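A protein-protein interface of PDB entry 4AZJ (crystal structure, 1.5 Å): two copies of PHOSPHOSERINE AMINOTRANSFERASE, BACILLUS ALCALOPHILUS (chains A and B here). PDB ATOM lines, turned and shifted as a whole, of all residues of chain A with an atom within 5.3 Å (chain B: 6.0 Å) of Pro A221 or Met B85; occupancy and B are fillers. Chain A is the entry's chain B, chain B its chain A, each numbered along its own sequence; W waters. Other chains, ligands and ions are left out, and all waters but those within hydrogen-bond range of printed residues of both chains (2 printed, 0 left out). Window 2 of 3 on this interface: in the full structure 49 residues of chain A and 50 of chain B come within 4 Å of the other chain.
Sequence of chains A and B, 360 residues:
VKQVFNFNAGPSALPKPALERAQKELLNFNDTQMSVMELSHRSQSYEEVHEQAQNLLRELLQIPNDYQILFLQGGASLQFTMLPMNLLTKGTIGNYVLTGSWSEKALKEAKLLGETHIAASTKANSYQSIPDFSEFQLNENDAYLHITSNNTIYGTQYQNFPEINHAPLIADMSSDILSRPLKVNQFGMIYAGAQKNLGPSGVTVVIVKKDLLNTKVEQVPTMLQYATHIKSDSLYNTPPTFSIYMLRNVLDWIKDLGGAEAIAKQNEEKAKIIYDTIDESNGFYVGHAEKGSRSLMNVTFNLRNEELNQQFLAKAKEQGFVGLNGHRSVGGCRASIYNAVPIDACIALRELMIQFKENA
OE2 of Glu B109 lies within hydrogen-bond range of OG1 of Thr A222, 2.6 Å away.
The backbone carbonyl oxygen (O) of Leu B224 sits at hydrogen-bond distance from the side-chain amide nitrogen (ND2) of Asn B86, at 2.8 Å.
Met A85 touches Pro B221. CE of Met A85 touches CD1 of Leu B224, 3.9 Å away. Gln A219 touches Leu B112 (OE1 to O, 3.7 Å). OG1 of Thr B81 touches CG of Pro A221, 3.3 Å away. CE of Met B85 touches CG of Pro A221 (3.7 Å). Glu B109 touches Pro A221 (OE1 to CA, 3.6 Å). CD1 of Leu A224 touches CD1 of Leu B224, 3.7 Å away.
Of the printed residues of chain B, Met A85 touches Pro B221 and Leu B224. Val A220 touches none of the printed residues of chain B. Printed residues of chain B within 4 Å of Pro A221: Thr B81 (3.3 Å), Met B85 (3.7 Å) and Glu B109 (3.6 Å). Printed residues of chain A within 4 Å of Thr B81: Pro A221 (3.3 Å). Of chain A, only Pro A221 comes within 4 Å of Met B85. Leu B88 touches none of the printed residues of chain A. Of the printed residues of chain A, Leu B112 touches Gln A219. Printed residues of chain A within 4 Å of Pro B221: Met A85 (3.7 Å). The nearest residue of chain A that does not touch Met B85 is Leu A224 (4.1 Å). The nearest printed residue of chain A that does not touch Glu B109 is Met A223 (4.8 Å).
Of the 8 printed residues of chain A, 5 touch a printed residue of chain B. Hydrophobic or aromatic side chains of chain A within 4 Å of the printed part of chain B: Met A85, Pro A221 and Leu A224. Of the 15 printed residues of chain B, 6 touch a printed residue of chain A. Printed residues of chain B that touch a printed residue of chain A: Thr B81, Met B85, Glu B109, Leu B112, Pro B221 and Leu B224. Hydrophobic or aromatic side chains of chain B within 4 Å of the printed part of chain A: Met B85, Pro B221 and Leu B224.
Met A85 touches Pro B221, and with the chains exchanged Pro A221 touches Met B85. Met A85 touches Leu B224, but with the chains exchanged Leu A224 does not touch Met B85 (4.1 Å). Leu B224 touches its own counterpart, Leu A224. Positions printed for both chains: 85, 220, 221 and 224. Of the 8 pairs that touch across the chains among the printed residues, 3 have their exchanged pair printed and touching as well.
Water W1 lies within hydrogen-bond range of N of Met A223 (2.8 Å), OE1 of Glu B109 (2.9 Å) and N of Thr A222 (3.2 Å). Water W2 bridges the backbone carbonyl oxygen (O) of Leu B112 (3.0 Å) and the side-chain amide oxygen (OE1) of Gln A219 (3.2 Å).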
ATOM      1  N   MET A  85     -12.719 -26.367   9.058  1.00  0.00           N
ATOM      2  CA  MET A  85     -13.076 -25.953   7.700  1.00  0.00           C
ATOM      3  C   MET A  85     -11.842 -25.882   6.831  1.00  0.00           C
ATOM      4  O   MET A  85     -11.919 -26.127   5.628  1.00  0.00           O
ATOM      5  CB  MET A  85     -13.698 -24.559   7.668  1.00  0.00           C
ATOM      6  CG  MET A  85     -15.107 -24.508   7.952  1.00  0.00           C
ATOM      7  SD  MET A  85     -15.771 -22.884   7.423  1.00  0.00           S
ATOM      8  CE  MET A  85     -17.334 -23.148   8.235  1.00  0.00           C
ATOM      9  N   GLN A 219     -13.765 -23.984  -1.860  1.00  0.00           N
ATOM     10  CA  GLN A 219     -15.150 -23.948  -1.427  1.00  0.00           C
ATOM     11  C   GLN A 219     -15.356 -23.333  -0.043  1.00  0.00           C
ATOM     12  O   GLN A 219     -16.479 -23.306   0.459  1.00  0.00           O
ATOM     13  CB  GLN A 219     -15.773 -25.349  -1.491  1.00  0.00           C
ATOM     14  CG  GLN A 219     -15.970 -25.846  -2.921  1.00  0.00           C
ATOM     15  CD  GLN A 219     -17.159 -25.184  -3.600  1.00  0.00           C
ATOM     16  OE1 GLN A 219     -18.309 -25.392  -3.199  1.00  0.00           O
ATOM     17  NE2 GLN A 219     -16.888 -24.371  -4.621  1.00  0.00           N
ATOM     18  N   VAL A 220     -14.290 -22.844   0.587  1.00  0.00           N
ATOM     19  CA  VAL A 220     -14.474 -22.241   1.901  1.00  0.00           C
ATOM     20  C   VAL A 220     -14.719 -20.754   1.736  1.00  0.00           C
ATOM     21  O   VAL A 220     -14.026 -20.100   0.987  1.00  0.00           O
ATOM     22  CB  VAL A 220     -13.261 -22.492   2.815  1.00  0.00           C
ATOM     23  CG1 VAL A 220     -13.379 -21.729   4.142  1.00  0.00           C
ATOM     24  CG2 VAL A 220     -13.134 -23.965   3.087  1.00  0.00           C
ATOM     25  N   PRO A 221     -15.721 -20.215   2.445  1.00  0.00           N
ATOM     26  CA  PRO A 221     -15.991 -18.781   2.333  1.00  0.00           C
ATOM     27  C   PRO A 221     -14.751 -17.950   2.606  1.00  0.00           C
ATOM     28  O   PRO A 221     -13.924 -18.291   3.449  1.00  0.00           O
ATOM     29  CB  PRO A 221     -17.049 -18.562   3.391  1.00  0.00           C
ATOM     30  CG  PRO A 221     -17.803 -19.871   3.410  1.00  0.00           C
ATOM     31  CD  PRO A 221     -16.738 -20.901   3.258  1.00  0.00           C
ATOM     32  N   THR A 222     -14.643 -16.849   1.872  1.00  0.00           N
ATOM     33  CA  THR A 222     -13.461 -16.005   1.926  1.00  0.00           C
ATOM     34  C   THR A 222     -13.056 -15.619   3.369  1.00  0.00           C
ATOM     35  O   THR A 222     -11.903 -15.722   3.738  1.00  0.00           O
ATOM     36  CB  THR A 222     -13.712 -14.737   1.129  1.00  0.00           C
ATOM     37  OG1 THR A 222     -14.104 -15.084  -0.201  1.00  0.00           O
ATOM     38  CG2 THR A 222     -12.450 -13.888   1.052  1.00  0.00           C
ATOM     39  N   MET A 223     -14.014 -15.193   4.171  1.00  0.00           N
ATOM     40  CA  MET A 223     -13.715 -14.777   5.544  1.00  0.00           C
ATOM     41  C   MET A 223     -13.268 -15.902   6.447  1.00  0.00           C
ATOM     42  O   MET A 223     -12.672 -15.661   7.512  1.00  0.00           O
ATOM     43  CB  MET A 223     -14.921 -14.102   6.198  1.00  0.00           C
ATOM     44  CG  MET A 223     -15.083 -12.631   5.821  1.00  0.00           C
ATOM     45  SD  MET A 223     -13.759 -11.598   6.499  1.00  0.00           S
ATOM     46  CE  MET A 223     -14.126 -11.604   8.236  1.00  0.00           C
ATOM     47  N   LEU A 224     -13.572 -17.131   6.037  1.00  0.00           N
ATOM     48  CA  LEU A 224     -13.272 -18.305   6.869  1.00  0.00           C
ATOM     49  C   LEU A 224     -12.036 -19.071   6.415  1.00  0.00           C
ATOM     50  O   LEU A 224     -11.724 -20.129   6.970  1.00  0.00           O
ATOM     51  CB  LEU A 224     -14.482 -19.225   6.897  1.00  0.00           C
ATOM     52  CG  LEU A 224     -15.681 -18.566   7.584  1.00  0.00           C
ATOM     53  CD1 LEU A 224     -16.962 -19.312   7.363  1.00  0.00           C
ATOM     54  CD2 LEU A 224     -15.400 -18.437   9.083  1.00  0.00           C
ATOM     55  N   GLN A 225     -11.304 -18.535   5.445  1.00  0.00           N
ATOM     56  CA  GLN A 225     -10.024 -19.098   5.041  1.00  0.00           C
ATOM     57  C   GLN A 225      -8.897 -18.440   5.814  1.00  0.00           C
ATOM     58  O   GLN A 225      -8.793 -17.209   5.807  1.00  0.00           O
ATOM     59  CB  GLN A 225      -9.751 -18.850   3.556  1.00  0.00           C
ATOM     60  CG  GLN A 225     -10.767 -19.500   2.655  1.00  0.00           C
ATOM     61  CD  GLN A 225     -10.343 -19.638   1.230  1.00  0.00           C
ATOM     62  OE1 GLN A 225      -9.156 -19.629   0.908  1.00  0.00           O
ATOM     63  NE2 GLN A 225     -11.309 -19.816   0.366  1.00  0.00           N
ATOM     64  N   THR B  81     -21.429 -14.158   3.865  1.00  0.00           N
ATOM     65  CA  THR B  81     -21.509 -15.625   3.803  1.00  0.00           C
ATOM     66  C   THR B  81     -22.580 -16.189   4.741  1.00  0.00           C
ATOM     67  O   THR B  81     -23.254 -17.160   4.392  1.00  0.00           O
ATOM     68  CB  THR B  81     -20.138 -16.315   4.020  1.00  0.00           C
ATOM     69  OG1 THR B  81     -20.261 -17.727   3.678  1.00  0.00           O
ATOM     70  CG2 THR B  81     -19.649 -16.233   5.440  1.00  0.00           C
ATOM     71  N   MET B  82     -22.764 -15.599   5.910  1.00  0.00           N
ATOM     72  CA  MET B  82     -23.729 -16.122   6.857  1.00  0.00           C
ATOM     73  C   MET B  82     -25.155 -16.068   6.301  1.00  0.00           C
ATOM     74  O   MET B  82     -25.951 -16.989   6.529  1.00  0.00           O
ATOM     75  CB  MET B  82     -23.617 -15.363   8.179  1.00  0.00           C
ATOM     76  CG  MET B  82     -24.264 -15.998   9.363  1.00  0.00           C
ATOM     77  SD  MET B  82     -23.741 -15.163  10.896  1.00  0.00           S
ATOM     78  CE  MET B  82     -24.911 -15.890  12.048  1.00  0.00           C
ATOM     79  N   LEU B  83     -25.494 -15.013   5.563  1.00  0.00           N
ATOM     80  CA  LEU B  83     -26.836 -14.903   4.978  1.00  0.00           C
ATOM     81  C   LEU B  83     -27.150 -16.090   4.045  1.00  0.00           C
ATOM     82  O   LEU B  83     -28.094 -16.837   4.318  1.00  0.00           O
ATOM     83  CB  LEU B  83     -27.023 -13.545   4.281  1.00  0.00           C
ATOM     84  CG  LEU B  83     -28.177 -13.508   3.255  1.00  0.00           C
ATOM     85  CD1 LEU B  83     -29.463 -13.551   4.041  1.00  0.00           C
ATOM     86  CD2 LEU B  83     -28.095 -12.279   2.368  1.00  0.00           C
ATOM     87  N   PRO B  84     -26.341 -16.336   3.020  1.00  0.00           N
ATOM     88  CA  PRO B  84     -26.666 -17.480   2.149  1.00  0.00           C
ATOM     89  C   PRO B  84     -26.520 -18.790   2.869  1.00  0.00           C
ATOM     90  O   PRO B  84     -27.263 -19.718   2.575  1.00  0.00           O
ATOM     91  CB  PRO B  84     -25.686 -17.350   0.987  1.00  0.00           C
ATOM     92  CG  PRO B  84     -24.585 -16.386   1.496  1.00  0.00           C
ATOM     93  CD  PRO B  84     -25.308 -15.472   2.428  1.00  0.00           C
ATOM     94  N   MET B  85     -25.597 -18.912   3.821  1.00  0.00           N
ATOM     95  CA  MET B  85     -25.516 -20.155   4.586  1.00  0.00           C
ATOM     96  C   MET B  85     -26.808 -20.500   5.252  1.00  0.00           C
ATOM     97  O   MET B  85     -27.119 -21.706   5.414  1.00  0.00           O
ATOM     98  CB  MET B  85     -24.482 -20.063   5.692  1.00  0.00           C
ATOM     99  CG  MET B  85     -23.174 -20.459   5.306  1.00  0.00           C
ATOM    100  SD  MET B  85     -22.078 -20.641   6.759  1.00  0.00           S
ATOM    101  CE  MET B  85     -20.579 -20.535   5.833  1.00  0.00           C
ATOM    102  N   ASN B  86     -27.531 -19.495   5.706  1.00  0.00           N
ATOM    103  CA  ASN B  86     -28.769 -19.695   6.412  1.00  0.00           C
ATOM    104  C   ASN B  86     -30.009 -19.781   5.530  1.00  0.00           C
ATOM    105  O   ASN B  86     -30.920 -20.561   5.826  1.00  0.00           O
ATOM    106  CB  ASN B  86     -28.971 -18.644   7.494  1.00  0.00           C
ATOM    107  CG  ASN B  86     -28.119 -18.907   8.701  1.00  0.00           C
ATOM    108  OD1 ASN B  86     -28.620 -19.338   9.753  1.00  0.00           O
ATOM    109  ND2 ASN B  86     -26.827 -18.660   8.566  1.00  0.00           N
ATOM    110  N   LEU B  87     -30.054 -19.022   4.446  1.00  0.00           N
ATOM    111  CA  LEU B  87     -31.287 -18.962   3.664  1.00  0.00           C
ATOM    112  C   LEU B  87     -31.205 -19.568   2.276  1.00  0.00           C
ATOM    113  O   LEU B  87     -32.258 -19.861   1.694  1.00  0.00           O
ATOM    114  CB  LEU B  87     -31.752 -17.513   3.519  1.00  0.00           C
ATOM    115  CG  LEU B  87     -32.396 -16.834   4.710  1.00  0.00           C
ATOM    116  CD1 LEU B  87     -32.885 -15.459   4.339  1.00  0.00           C
ATOM    117  CD2 LEU B  87     -33.558 -17.628   5.296  1.00  0.00           C
ATOM    118  N   LEU B  88     -30.011 -19.716   1.720  1.00  0.00           N
ATOM    119  CA  LEU B  88     -29.857 -20.170   0.356  1.00  0.00           C
ATOM    120  C   LEU B  88     -29.790 -21.677   0.357  1.00  0.00           C
ATOM    121  O   LEU B  88     -28.734 -22.284   0.424  1.00  0.00           O
ATOM    122  CB  LEU B  88     -28.632 -19.550  -0.328  1.00  0.00           C
ATOM    123  CG  LEU B  88     -28.378 -19.926  -1.786  1.00  0.00           C
ATOM    124  CD1 LEU B  88     -29.615 -19.747  -2.606  1.00  0.00           C
ATOM    125  CD2 LEU B  88     -27.254 -19.074  -2.369  1.00  0.00           C
ATOM    126  N   GLU B 109     -19.902 -14.276  -2.277  1.00  0.00           N
ATOM    127  CA  GLU B 109     -19.980 -15.283  -1.222  1.00  0.00           C
ATOM    128  C   GLU B 109     -21.180 -16.193  -1.403  1.00  0.00           C
ATOM    129  O   GLU B 109     -21.080 -17.389  -1.122  1.00  0.00           O
ATOM    130  CB  GLU B 109     -19.976 -14.602   0.155  1.00  0.00           C
ATOM    131  CG  GLU B 109     -18.706 -13.833   0.436  1.00  0.00           C
ATOM    132  CD  GLU B 109     -17.429 -14.651   0.262  1.00  0.00           C
ATOM    133  OE1 GLU B 109     -17.356 -15.794   0.788  1.00  0.00           O
ATOM    134  OE2 GLU B 109     -16.488 -14.175  -0.402  1.00  0.00           O
ATOM    135  N   LEU B 112     -20.552 -19.168  -3.921  1.00  0.00           N
ATOM    136  CA  LEU B 112     -19.865 -20.328  -3.358  1.00  0.00           C
ATOM    137  C   LEU B 112     -20.838 -21.336  -2.760  1.00  0.00           C
ATOM    138  O   LEU B 112     -20.533 -22.531  -2.689  1.00  0.00           O
ATOM    139  CB  LEU B 112     -18.838 -19.906  -2.286  1.00  0.00           C
ATOM    140  CG  LEU B 112     -17.662 -19.081  -2.799  1.00  0.00           C
ATOM    141  CD1 LEU B 112     -16.782 -18.545  -1.652  1.00  0.00           C
ATOM    142  CD2 LEU B 112     -16.822 -19.894  -3.773  1.00  0.00           C
ATOM    143  N   LEU B 113     -22.016 -20.879  -2.322  1.00  0.00           N
ATOM    144  CA  LEU B 113     -22.930 -21.725  -1.565  1.00  0.00           C
ATOM    145  C   LEU B 113     -24.187 -22.212  -2.285  1.00  0.00           C
ATOM    146  O   LEU B 113     -24.902 -23.084  -1.771  1.00  0.00           O
ATOM    147  CB  LEU B 113     -23.363 -20.956  -0.312  1.00  0.00           C
ATOM    148  CG  LEU B 113     -22.144 -20.548   0.514  1.00  0.00           C
ATOM    149  CD1 LEU B 113     -22.565 -19.601   1.616  1.00  0.00           C
ATOM    150  CD2 LEU B 113     -21.404 -21.759   1.069  1.00  0.00           C
ATOM    151  N   VAL B 217     -30.413 -24.452  10.984  1.00  0.00           N
ATOM    152  CA  VAL B 217     -30.042 -24.899   9.655  1.00  0.00           C
ATOM    153  C   VAL B 217     -29.178 -26.127   9.619  1.00  0.00           C
ATOM    154  O   VAL B 217     -28.088 -26.097  10.223  1.00  0.00           O
ATOM    155  CB  VAL B 217     -29.600 -23.773   8.653  1.00  0.00           C
ATOM    156  CG1 VAL B 217     -29.442 -24.301   7.255  1.00  0.00           C
ATOM    157  CG2 VAL B 217     -30.521 -22.566   8.707  1.00  0.00           C
ATOM    158  N   VAL B 220     -25.019 -26.408   9.347  1.00  0.00           N
ATOM    159  CA  VAL B 220     -24.331 -25.123   9.449  1.00  0.00           C
ATOM    160  C   VAL B 220     -23.644 -25.036  10.825  1.00  0.00           C
ATOM    161  O   VAL B 220     -24.246 -25.340  11.851  1.00  0.00           O
ATOM    162  CB  VAL B 220     -25.308 -23.973   9.244  1.00  0.00           C
ATOM    163  CG1 VAL B 220     -24.652 -22.593   9.579  1.00  0.00           C
ATOM    164  CG2 VAL B 220     -25.815 -23.972   7.813  1.00  0.00           C
ATOM    165  N   PRO B 221     -22.368 -24.624  10.844  1.00  0.00           N
ATOM    166  CA  PRO B 221     -21.700 -24.438  12.140  1.00  0.00           C
ATOM    167  C   PRO B 221     -22.483 -23.583  13.119  1.00  0.00           C
ATOM    168  O   PRO B 221     -23.139 -22.614  12.744  1.00  0.00           O
ATOM    169  CB  PRO B 221     -20.397 -23.742  11.747  1.00  0.00           C
ATOM    170  CG  PRO B 221     -20.081 -24.254  10.374  1.00  0.00           C
ATOM    171  CD  PRO B 221     -21.468 -24.333   9.712  1.00  0.00           C
ATOM    172  N   LEU B 224     -22.376 -19.832  13.045  1.00  0.00           N
ATOM    173  CA  LEU B 224     -22.797 -19.245  11.772  1.00  0.00           C
ATOM    174  C   LEU B 224     -24.312 -19.409  11.555  1.00  0.00           C
ATOM    175  O   LEU B 224     -24.811 -19.086  10.478  1.00  0.00           O
ATOM    176  CB  LEU B 224     -21.986 -19.829  10.611  1.00  0.00           C
ATOM    177  CG  LEU B 224     -20.485 -19.532  10.664  1.00  0.00           C
ATOM    178  CD1 LEU B 224     -19.709 -20.361   9.639  1.00  0.00           C
ATOM    179  CD2 LEU B 224     -20.243 -18.041  10.479  1.00  0.00           C
HETATM  180  O   HOH W   1     -16.739 -14.964   3.484  1.00  0.00           O
HETATM  181  O   HOH W   2     -20.658 -25.055  -1.085  1.00  0.00           O
